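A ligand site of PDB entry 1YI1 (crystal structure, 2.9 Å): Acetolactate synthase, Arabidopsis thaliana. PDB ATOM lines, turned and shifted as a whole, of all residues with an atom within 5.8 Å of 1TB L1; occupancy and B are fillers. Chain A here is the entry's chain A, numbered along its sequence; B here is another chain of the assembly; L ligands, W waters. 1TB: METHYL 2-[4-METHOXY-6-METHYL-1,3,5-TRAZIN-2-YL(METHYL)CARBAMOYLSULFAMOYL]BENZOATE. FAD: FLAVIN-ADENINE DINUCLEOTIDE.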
ATOM      1  N   MET A 266      10.689  14.603   1.148  1.00  0.00           N
ATOM      2  CA  MET A 266      11.521  13.438   1.390  1.00  0.00           C
ATOM      3  C   MET A 266      12.180  12.904   0.131  1.00  0.00           C
ATOM      4  O   MET A 266      13.333  12.476   0.143  1.00  0.00           O
ATOM      5  CB  MET A 266      10.669  12.330   2.029  1.00  0.00           C
ATOM      6  CG  MET A 266      11.346  10.996   2.141  1.00  0.00           C
ATOM      7  SD  MET A 266      10.353   9.880   3.128  1.00  0.00           S
ATOM      8  CE  MET A 266      10.886  10.398   4.780  1.00  0.00           C
ATOM      9  N   HIS A 267      11.431  12.957  -0.977  1.00  0.00           N
ATOM     10  CA  HIS A 267      11.935  12.496  -2.259  1.00  0.00           C
ATOM     11  C   HIS A 267      11.934  13.619  -3.283  1.00  0.00           C
ATOM     12  O   HIS A 267      11.859  13.379  -4.482  1.00  0.00           O
ATOM     13  CB  HIS A 267      11.079  11.336  -2.752  1.00  0.00           C
ATOM     14  CG  HIS A 267      11.279  10.075  -1.992  1.00  0.00           C
ATOM     15  ND1 HIS A 267      12.478   9.400  -1.969  1.00  0.00           N
ATOM     16  CD2 HIS A 267      10.437   9.366  -1.198  1.00  0.00           C
ATOM     17  CE1 HIS A 267      12.374   8.333  -1.195  1.00  0.00           C
ATOM     18  NE2 HIS A 267      11.143   8.287  -0.722  1.00  0.00           N
ATOM     19  N   ASP A 291       4.877  16.311   7.259  1.00  0.00           N
ATOM     20  CA  ASP A 291       6.209  15.882   7.671  1.00  0.00           C
ATOM     21  C   ASP A 291       7.047  15.307   6.516  1.00  0.00           C
ATOM     22  O   ASP A 291       8.272  15.385   6.554  1.00  0.00           O
ATOM     23  CB  ASP A 291       6.133  14.859   8.830  1.00  0.00           C
ATOM     24  CG  ASP A 291       5.461  13.562   8.436  1.00  0.00           C
ATOM     25  OD1 ASP A 291       4.211  13.519   8.350  1.00  0.00           O
ATOM     26  OD2 ASP A 291       6.194  12.584   8.208  1.00  0.00           O
ATOM     27  N   ARG A 292       6.391  14.760   5.492  1.00  0.00           N
ATOM     28  CA  ARG A 292       7.153  14.235   4.359  1.00  0.00           C
ATOM     29  C   ARG A 292       7.701  15.412   3.569  1.00  0.00           C
ATOM     30  O   ARG A 292       8.316  15.235   2.521  1.00  0.00           O
ATOM     31  CB  ARG A 292       6.287  13.371   3.429  1.00  0.00           C
ATOM     32  CG  ARG A 292       5.308  12.465   4.118  1.00  0.00           C
ATOM     33  CD  ARG A 292       5.920  11.816   5.336  1.00  0.00           C
ATOM     34  NE  ARG A 292       6.715  10.646   5.003  1.00  0.00           N
ATOM     35  CZ  ARG A 292       7.273   9.864   5.920  1.00  0.00           C
ATOM     36  NH1 ARG A 292       7.109  10.130   7.212  1.00  0.00           N
ATOM     37  NH2 ARG A 292       7.969   8.796   5.545  1.00  0.00           N
ATOM     38  N   MET A 485       8.791   0.144  -1.984  1.00  0.00           N
ATOM     39  CA  MET A 485       9.092   1.124  -0.954  1.00  0.00           C
ATOM     40  C   MET A 485       9.490   0.520   0.378  1.00  0.00           C
ATOM     41  O   MET A 485      10.389   1.009   1.039  1.00  0.00           O
ATOM     42  CB  MET A 485       7.919   2.084  -0.759  1.00  0.00           C
ATOM     43  CG  MET A 485       8.296   3.329   0.049  1.00  0.00           C
ATOM     44  SD  MET A 485       9.828   4.102  -0.531  1.00  0.00           S
ATOM     45  CE  MET A 485       9.270   4.879  -2.021  1.00  0.00           C
ATOM     46  N   VAL A 486       8.802  -0.548   0.780  1.00  0.00           N
ATOM     47  CA  VAL A 486       9.159  -1.178   2.043  1.00  0.00           C
ATOM     48  C   VAL A 486      10.537  -1.826   1.884  1.00  0.00           C
ATOM     49  O   VAL A 486      11.366  -1.767   2.783  1.00  0.00           O
ATOM     50  CB  VAL A 486       8.134  -2.257   2.442  1.00  0.00           C
ATOM     51  CG1 VAL A 486       8.490  -2.851   3.790  1.00  0.00           C
ATOM     52  CG2 VAL A 486       6.748  -1.638   2.494  1.00  0.00           C
ATOM     53  N   TRP A 489      13.466   0.448   2.256  1.00  0.00           N
ATOM     54  CA  TRP A 489      13.738   0.763   3.648  1.00  0.00           C
ATOM     55  C   TRP A 489      14.478  -0.388   4.340  1.00  0.00           C
ATOM     56  O   TRP A 489      15.301  -0.163   5.223  1.00  0.00           O
ATOM     57  CB  TRP A 489      12.439   1.128   4.385  1.00  0.00           C
ATOM     58  CG  TRP A 489      12.050   2.595   4.208  1.00  0.00           C
ATOM     59  CD1 TRP A 489      11.850   3.258   3.031  1.00  0.00           C
ATOM     60  CD2 TRP A 489      11.891   3.565   5.248  1.00  0.00           C
ATOM     61  NE1 TRP A 489      11.591   4.584   3.274  1.00  0.00           N
ATOM     62  CE2 TRP A 489      11.602   4.803   4.619  1.00  0.00           C
ATOM     63  CE3 TRP A 489      11.961   3.520   6.649  1.00  0.00           C
ATOM     64  CZ2 TRP A 489      11.396   5.982   5.352  1.00  0.00           C
ATOM     65  CZ3 TRP A 489      11.751   4.694   7.363  1.00  0.00           C
ATOM     66  CH2 TRP A 489      11.469   5.907   6.719  1.00  0.00           C
ATOM     67  N   SER A 568      13.182  10.109   7.294  1.00  0.00           N
ATOM     68  CA  SER A 568      12.119  10.640   8.136  1.00  0.00           C
ATOM     69  C   SER A 568      12.586  11.493   9.318  1.00  0.00           C
ATOM     70  O   SER A 568      13.310  11.019  10.195  1.00  0.00           O
ATOM     71  CB  SER A 568      11.270   9.465   8.656  1.00  0.00           C
ATOM     72  OG  SER A 568      10.015   9.908   9.138  1.00  0.00           O
ATOM     73  N   GLY A 569      12.162  12.754   9.326  1.00  0.00           N
ATOM     74  CA  GLY A 569      12.535  13.665  10.404  1.00  0.00           C
ATOM     75  C   GLY A 569      13.919  14.265  10.256  1.00  0.00           C
ATOM     76  O   GLY A 569      14.478  14.777  11.224  1.00  0.00           O
ATOM     77  N   GLY B  35       4.182  -3.005   6.285  1.00  0.00           N
ATOM     78  CA  GLY B  35       3.992  -1.603   5.981  1.00  0.00           C
ATOM     79  C   GLY B  35       5.015  -0.814   6.784  1.00  0.00           C
ATOM     80  O   GLY B  35       5.528  -1.292   7.789  1.00  0.00           O
ATOM     81  N   GLY B  36       5.312   0.410   6.350  1.00  0.00           N
ATOM     82  CA  GLY B  36       6.287   1.218   7.061  1.00  0.00           C
ATOM     83  C   GLY B  36       6.154   1.287   8.576  1.00  0.00           C
ATOM     84  O   GLY B  36       7.137   1.129   9.286  1.00  0.00           O
ATOM     85  N   ALA B  37       4.941   1.528   9.078  1.00  0.00           N
ATOM     86  CA  ALA B  37       4.737   1.652  10.516  1.00  0.00           C
ATOM     87  C   ALA B  37       4.906   0.348  11.305  1.00  0.00           C
ATOM     88  O   ALA B  37       5.074   0.372  12.518  1.00  0.00           O
ATOM     89  CB  ALA B  37       3.362   2.236  10.800  1.00  0.00           C
ATOM     90  N   MET B  39       7.193  -2.239  10.190  1.00  0.00           N
ATOM     91  CA  MET B  39       8.412  -2.943   9.793  1.00  0.00           C
ATOM     92  C   MET B  39       9.082  -3.684  10.952  1.00  0.00           C
ATOM     93  O   MET B  39       9.332  -4.880  10.874  1.00  0.00           O
ATOM     94  CB  MET B  39       9.399  -1.972   9.147  1.00  0.00           C
ATOM     95  CG  MET B  39       8.967  -1.504   7.777  1.00  0.00           C
ATOM     96  SD  MET B  39      10.217  -0.509   6.954  1.00  0.00           S
ATOM     97  CE  MET B  39      11.174  -1.765   6.125  1.00  0.00           C
ATOM     98  N   THR B  82      -0.213  -2.563   9.141  1.00  0.00           N
ATOM     99  CA  THR B  82       0.514  -1.329   9.361  1.00  0.00           C
ATOM    100  C   THR B  82      -0.465  -0.195   9.699  1.00  0.00           C
ATOM    101  O   THR B  82      -1.670  -0.418   9.806  1.00  0.00           O
ATOM    102  CB  THR B  82       1.349  -0.966   8.119  1.00  0.00           C
ATOM    103  OG1 THR B  82       2.154   0.188   8.400  1.00  0.00           O
ATOM    104  CG2 THR B  82       0.453  -0.689   6.931  1.00  0.00           C
ATOM    105  N   SER B  83       0.056   1.005   9.865  1.00  0.00           N
ATOM    106  CA  SER B  83      -0.769   2.150  10.179  1.00  0.00           C
ATOM    107  C   SER B  83      -1.632   2.562   8.998  1.00  0.00           C
ATOM    108  O   SER B  83      -1.610   1.920   7.952  1.00  0.00           O
ATOM    109  CB  SER B  83       0.119   3.320  10.599  1.00  0.00           C
ATOM    110  OG  SER B  83       0.966   3.702   9.539  1.00  0.00           O
ATOM    111  N   GLN B 110       1.371   1.916  14.376  1.00  0.00           N
ATOM    112  CA  GLN B 110       0.848   3.263  14.421  1.00  0.00           C
ATOM    113  C   GLN B 110       2.031   4.205  14.318  1.00  0.00           C
ATOM    114  O   GLN B 110       3.169   3.793  14.519  1.00  0.00           O
ATOM    115  CB  GLN B 110       0.096   3.509  15.732  1.00  0.00           C
ATOM    116  CG  GLN B 110      -0.389   4.929  15.885  1.00  0.00           C
ATOM    117  CD  GLN B 110      -1.296   5.349  14.742  1.00  0.00           C
ATOM    118  OE1 GLN B 110      -2.512   5.163  14.798  1.00  0.00           O
ATOM    119  NE2 GLN B 110      -0.706   5.904  13.694  1.00  0.00           N
ATOM    120  N   VAL B 111       1.765   5.462  13.976  1.00  0.00           N
ATOM    121  CA  VAL B 111       2.822   6.449  13.864  1.00  0.00           C
ATOM    122  C   VAL B 111       3.426   6.664  15.262  1.00  0.00           C
ATOM    123  O   VAL B 111       2.847   6.228  16.272  1.00  0.00           O
ATOM    124  CB  VAL B 111       2.247   7.786  13.359  1.00  0.00           C
ATOM    125  CG1 VAL B 111       1.717   7.609  11.957  1.00  0.00           C
ATOM    126  CG2 VAL B 111       1.149   8.267  14.297  1.00  0.00           C
ATOM    127  N   PRO B 112       4.595   7.307  15.345  1.00  0.00           N
ATOM    128  CA  PRO B 112       5.230   7.548  16.644  1.00  0.00           C
ATOM    129  C   PRO B 112       4.246   8.261  17.554  1.00  0.00           C
ATOM    130  O   PRO B 112       3.390   9.004  17.081  1.00  0.00           O
ATOM    131  CB  PRO B 112       6.419   8.424  16.283  1.00  0.00           C
ATOM    132  CG  PRO B 112       6.800   7.927  14.930  1.00  0.00           C
ATOM    133  CD  PRO B 112       5.453   7.792  14.242  1.00  0.00           C
ATOM    134  N   ARG B 114       4.421  10.869  19.581  1.00  0.00           N
ATOM    135  CA  ARG B 114       4.401  12.323  19.461  1.00  0.00           C
ATOM    136  C   ARG B 114       3.697  12.823  18.200  1.00  0.00           C
ATOM    137  O   ARG B 114       3.171  13.938  18.187  1.00  0.00           O
ATOM    138  CB  ARG B 114       5.832  12.887  19.484  1.00  0.00           C
ATOM    139  CG  ARG B 114       6.722  12.300  18.417  1.00  0.00           C
ATOM    140  CD  ARG B 114       7.814  13.266  18.016  1.00  0.00           C
ATOM    141  NE  ARG B 114       8.423  12.868  16.748  1.00  0.00           N
ATOM    142  CZ  ARG B 114       9.063  13.706  15.924  1.00  0.00           C
ATOM    143  NH1 ARG B 114       9.189  14.989  16.240  1.00  0.00           N
ATOM    144  NH2 ARG B 114       9.554  13.246  14.772  1.00  0.00           N
ATOM    145  N   MET B 115       3.670  12.006  17.152  1.00  0.00           N
ATOM    146  CA  MET B 115       3.022  12.358  15.882  1.00  0.00           C
ATOM    147  C   MET B 115       1.513  12.155  15.874  1.00  0.00           C
ATOM    148  O   MET B 115       0.808  12.674  15.012  1.00  0.00           O
ATOM    149  CB  MET B 115       3.608  11.528  14.747  1.00  0.00           C
ATOM    150  CG  MET B 115       5.056  11.799  14.428  1.00  0.00           C
ATOM    151  SD  MET B 115       5.285  13.323  13.504  1.00  0.00           S
ATOM    152  CE  MET B 115       6.279  14.250  14.665  1.00  0.00           C
ATOM    153  N   ALA B 120      -0.483  13.055  10.526  1.00  0.00           N
ATOM    154  CA  ALA B 120       0.809  12.542  10.121  1.00  0.00           C
ATOM    155  C   ALA B 120       0.655  11.595   8.957  1.00  0.00           C
ATOM    156  O   ALA B 120      -0.445  11.135   8.634  1.00  0.00           O
ATOM    157  CB  ALA B 120       1.479  11.835  11.269  1.00  0.00           C
ATOM    158  N   PHE B 121       1.783  11.283   8.334  1.00  0.00           N
ATOM    159  CA  PHE B 121       1.807  10.382   7.205  1.00  0.00           C
ATOM    160  C   PHE B 121       1.275   9.013   7.612  1.00  0.00           C
ATOM    161  O   PHE B 121       1.700   8.443   8.621  1.00  0.00           O
ATOM    162  CB  PHE B 121       3.230  10.249   6.693  1.00  0.00           C
ATOM    163  CG  PHE B 121       3.404   9.230   5.622  1.00  0.00           C
ATOM    164  CD1 PHE B 121       2.774   9.382   4.397  1.00  0.00           C
ATOM    165  CD2 PHE B 121       4.206   8.111   5.835  1.00  0.00           C
ATOM    166  CE1 PHE B 121       2.937   8.437   3.391  1.00  0.00           C
ATOM    167  CE2 PHE B 121       4.378   7.161   4.830  1.00  0.00           C
ATOM    168  CZ  PHE B 121       3.739   7.334   3.610  1.00  0.00           C
ATOM    169  N   GLN B 122       0.329   8.491   6.831  1.00  0.00           N
ATOM    170  CA  GLN B 122      -0.275   7.191   7.074  1.00  0.00           C
ATOM    171  C   GLN B 122      -0.866   6.917   8.464  1.00  0.00           C
ATOM    172  O   GLN B 122      -0.725   5.798   8.980  1.00  0.00           O
ATOM    173  CB  GLN B 122       0.716   6.076   6.738  1.00  0.00           C
ATOM    174  CG  GLN B 122       1.118   6.025   5.281  1.00  0.00           C
ATOM    175  CD  GLN B 122       1.657   4.664   4.875  1.00  0.00           C
ATOM    176  OE1 GLN B 122       2.613   4.152   5.473  1.00  0.00           O
ATOM    177  NE2 GLN B 122       1.054   4.070   3.856  1.00  0.00           N
ATOM    178  N   LYS B 171       5.132   3.233  16.384  1.00  0.00           N
ATOM    179  CA  LYS B 171       6.439   2.898  15.849  1.00  0.00           C
ATOM    180  C   LYS B 171       7.576   3.120  16.840  1.00  0.00           C
ATOM    181  O   LYS B 171       8.465   2.281  16.974  1.00  0.00           O
ATOM    182  CB  LYS B 171       6.715   3.700  14.567  1.00  0.00           C
ATOM    183  CG  LYS B 171       8.118   3.520  14.030  1.00  0.00           C
ATOM    184  CD  LYS B 171       8.131   3.681  12.524  1.00  0.00           C
ATOM    185  CE  LYS B 171       9.529   3.460  11.979  1.00  0.00           C
ATOM    186  NZ  LYS B 171      10.493   4.409  12.609  1.00  0.00           N
HETATM  187  C4  1TB L   1       6.154  11.033  10.971  1.00  0.00           C
HETATM  188  C5  1TB L   1       4.715  10.595  10.541  1.00  0.00           C
HETATM  189  C6  1TB L   1       4.400   9.128  10.243  1.00  0.00           C
HETATM  190  C1  1TB L   1       5.501   8.034  10.368  1.00  0.00           C
HETATM  191  C2  1TB L   1       6.938   8.505  10.811  1.00  0.00           C
HETATM  192  C3  1TB L   1       7.255  10.009  11.108  1.00  0.00           C
HETATM  193  C11 1TB L   1       5.169   6.595  10.076  1.00  0.00           C
HETATM  194  O12 1TB L   1       4.858   6.174   8.766  1.00  0.00           O
HETATM  195  C13 1TB L   1       4.531   4.967   8.213  1.00  0.00           C
HETATM  196  O11 1TB L   1       5.173   5.651  11.099  1.00  0.00           O
HETATM  197  S7  1TB L   1       8.285   7.344  10.970  1.00  0.00           S
HETATM  198  N8  1TB L   1       8.304   6.227  10.023  1.00  0.00           N
HETATM  199  C9  1TB L   1       8.250   6.259   8.558  1.00  0.00           C
HETATM  200  O7A 1TB L   1       8.324   6.766  12.291  1.00  0.00           O
HETATM  201  O7B 1TB L   1       9.528   8.056  10.795  1.00  0.00           O
HETATM  202  O9  1TB L   1       8.156   7.445   7.916  1.00  0.00           O
HETATM  203  N10 1TB L   1       8.285   4.976   7.848  1.00  0.00           N
HETATM  204  C2' 1TB L   1       8.220   4.834   6.384  1.00  0.00           C
HETATM  205  N1' 1TB L   1       8.270   3.556   5.798  1.00  0.00           N
HETATM  206  C6' 1TB L   1       8.203   3.360   4.414  1.00  0.00           C
HETATM  207  N5' 1TB L   1       8.095   4.490   3.622  1.00  0.00           N
HETATM  208  C4' 1TB L   1       8.049   5.773   4.164  1.00  0.00           C
HETATM  209  N3' 1TB L   1       8.117   5.917   5.520  1.00  0.00           N
HETATM  210  C10 1TB L   1       8.398   3.767   8.705  1.00  0.00           C
HETATM  211  O4' 1TB L   1       7.956   6.838   3.484  1.00  0.00           O
HETATM  212  C5' 1TB L   1       7.862   7.356   2.265  1.00  0.00           C
HETATM  213  C7' 1TB L   1       8.269   1.878   3.864  1.00  0.00           C
HETATM  214  PA  FAD L   2      -2.971  18.709   0.815  1.00  0.00           P
HETATM  215  O1A FAD L   2      -3.988  18.464  -0.246  1.00  0.00           O
HETATM  216  O2A FAD L   2      -2.624  17.694   1.780  1.00  0.00           O
HETATM  217  O5B FAD L   2      -3.283  19.911   1.668  1.00  0.00           O
HETATM  218  C5B FAD L   2      -3.770  21.129   1.001  1.00  0.00           C
HETATM  219  C4B FAD L   2      -3.920  22.215   2.025  1.00  0.00           C
HETATM  220  O4B FAD L   2      -4.407  23.326   1.262  1.00  0.00           O
HETATM  221  C3B FAD L   2      -4.903  22.146   3.285  1.00  0.00           C
HETATM  222  O3B FAD L   2      -4.390  22.682   4.499  1.00  0.00           O
HETATM  223  C2B FAD L   2      -6.145  22.755   2.716  1.00  0.00           C
HETATM  224  O2B FAD L   2      -7.246  22.968   3.512  1.00  0.00           O
HETATM  225  C1B FAD L   2      -5.506  23.908   1.927  1.00  0.00           C
HETATM  226  N9A FAD L   2      -6.387  24.539   0.832  1.00  0.00           N
HETATM  227  C8A FAD L   2      -7.308  23.703   0.055  1.00  0.00           C
HETATM  228  N7A FAD L   2      -8.011  24.313  -0.835  1.00  0.00           N
HETATM  229  C5A FAD L   2      -7.646  25.604  -0.739  1.00  0.00           C
HETATM  230  C6A FAD L   2      -7.996  26.964  -1.424  1.00  0.00           C
HETATM  231  N6A FAD L   2      -8.884  27.011  -2.385  1.00  0.00           N
HETATM  232  N1A FAD L   2      -7.325  28.190  -0.988  1.00  0.00           N
HETATM  233  C2A FAD L   2      -6.343  28.174   0.073  1.00  0.00           C
HETATM  234  N3A FAD L   2      -5.957  27.004   0.747  1.00  0.00           N
HETATM  235  C4A FAD L   2      -6.612  25.748   0.327  1.00  0.00           C
HETATM  236  N1  FAD L   2       4.781  14.811  -0.435  1.00  0.00           N
HETATM  237  C2  FAD L   2       5.723  15.667  -0.794  1.00  0.00           C
HETATM  238  O2  FAD L   2       5.366  16.812  -1.062  1.00  0.00           O
HETATM  239  N3  FAD L   2       7.061  15.275  -0.968  1.00  0.00           N
HETATM  240  C4  FAD L   2       7.480  13.921  -0.809  1.00  0.00           C
HETATM  241  O4  FAD L   2       8.673  13.584  -0.853  1.00  0.00           O
HETATM  242  C4X FAD L   2       6.419  12.946  -0.498  1.00  0.00           C
HETATM  243  N5  FAD L   2       6.729  11.610  -0.386  1.00  0.00           N
HETATM  244  C5X FAD L   2       5.701  10.718  -0.127  1.00  0.00           C
HETATM  245  C6  FAD L   2       5.997   9.325  -0.197  1.00  0.00           C
HETATM  246  C7  FAD L   2       4.943   8.358  -0.123  1.00  0.00           C
HETATM  247  C7M FAD L   2       5.285   6.908  -0.367  1.00  0.00           C
HETATM  248  C8  FAD L   2       3.560   8.809   0.085  1.00  0.00           C
HETATM  249  C8M FAD L   2       2.361   7.860   0.055  1.00  0.00           C
HETATM  250  C9  FAD L   2       3.292  10.189   0.228  1.00  0.00           C
HETATM  251  C9A FAD L   2       4.309  11.172   0.071  1.00  0.00           C
HETATM  252  N10 FAD L   2       4.066  12.570   0.088  1.00  0.00           N
HETATM  253  C10 FAD L   2       5.062  13.468  -0.295  1.00  0.00           C
HETATM  254  C1' FAD L   2       2.645  13.085   0.114  1.00  0.00           C
HETATM  255  C2' FAD L   2       2.448  13.550   1.481  1.00  0.00           C
HETATM  256  O2' FAD L   2       2.027  12.502   2.355  1.00  0.00           O
HETATM  257  C3' FAD L   2       1.391  14.657   1.663  1.00  0.00           C
HETATM  258  O3' FAD L   2       0.137  14.062   1.051  1.00  0.00           O
HETATM  259  C4' FAD L   2       1.598  15.976   0.857  1.00  0.00           C
HETATM  260  O4' FAD L   2       2.937  16.534   1.315  1.00  0.00           O
HETATM  261  C5' FAD L   2       0.537  16.923   1.203  1.00  0.00           C
HETATM  262  O5' FAD L   2       0.792  18.137   0.441  1.00  0.00           O
HETATM  263  P   FAD L   2      -0.139  19.388   0.533  1.00  0.00           P
HETATM  264  O1P FAD L   2      -0.109  19.812   1.963  1.00  0.00           O
HETATM  265  O2P FAD L   2       0.458  20.340  -0.338  1.00  0.00           O
HETATM  266  O3P FAD L   2      -1.612  19.057   0.024  1.00  0.00           O
HETATM  267  O   HOH W   1      10.634   6.352   0.976  1.00  0.00           O
HETATM  268  O   HOH W   2      10.503   7.863  14.523  1.00  0.00           O
HETATM  269  O   HOH W   3       9.819  11.249  12.773  1.00  0.00           O
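The side-chain hydroxyl (OG) of Ser 568 lies within hydrogen-bond range of the guanidinium group (NH1) of Arg 292, at 3.5 Å. The guanidinium group (NH1) of Arg 292 is in salt-bridge range of the side-chain carboxylate (OD2) of Asp 291 (2.8 Å). O of Arg 292 lies within hydrogen-bond range of N of Met 266. The side-chain carboxylate of Asp 291 sits at hydrogen-bond distance from the backbone NH of Phe 121 of chain B, at 3.3 Å. The backbone carbonyl oxygen (O) of Gln 122 of chain B sits at hydrogen-bond distance from the side-chain hydroxyl (OG) of Ser 83 of chain B (2.8 Å). The side-chain hydroxyl of Thr 82 of chain B lies within hydrogen-bond range of the backbone NH of Ala 37 of chain B (3.2 Å).
The side-chain hydroxyl (OG) of Ser 568 is in hydrogen-bond range of an oxygen (O7B) of 1TB L1, 2.5 Å away. O9 of 1TB L1 lies within hydrogen-bond range of NH2 of Arg 292, at 2.7 Å. The side-chain amino group (NZ) of Lys 171 of chain B sits close to an oxygen (O7A) of 1TB L1 (3.2 Å). The backbone NH of Met 266 is in hydrogen-bond range of an oxygen (O4) of FAD L2 (3.0 Å). The backbone NH (N) of His 267 sits at hydrogen-bond distance from an oxygen (O4) of FAD L2 (2.8 Å).
Merely in contact with 1TB L1: Met 266 (3.6 Å), Asp 291 (3.2 Å), Met 485 (3.6 Å), Val 486 (3.7 Å), Trp 489 (3.3 Å), Gly 36 of chain B (3.0 Å), Ala 37 of chain B (3.6 Å), Val 111 of chain B (3.5 Å), Pro 112 of chain B (3.3 Å), Met 115 of chain B (3.5 Å), Ala 120 of chain B (3.5 Å), Phe 121 of chain B (3.2 Å) and Gln 122 of chain B (3.4 Å). Hydrophobic or aromatic side chains within 4 Å of 1TB L1: Met 266, Met 485, Trp 489, Ala 37 of chain B, Val 111 of chain B, Pro 112 of chain B, Met 115 of chain B, Ala 120 of chain B and Phe 121 of chain B. 16 residues have an atom within 4 Å of 1TB L1: Met 266, Asp 291, Arg 292, Met 485, Val 486, Trp 489, Ser 568, Gly 36 of chain B, Ala 37 of chain B, Val 111 of chain B, Pro 112 of chain B, Met 115 of chain B, Ala 120 of chain B, Phe 121 of chain B, Gln 122 of chain B and Lys 171 of chain B. The nearest printed residue that does not touch 1TB L1 is Ser 83 of chain B (4.01 Å).
Water W1 lies within hydrogen-bond range of a ring nitrogen (NE2) of His 267 (2.6 Å), the side-chain sulfur (SD) of Met 485 (2.8 Å) and the indole nitrogen (NE1) of Trp 489 (3.1 Å).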
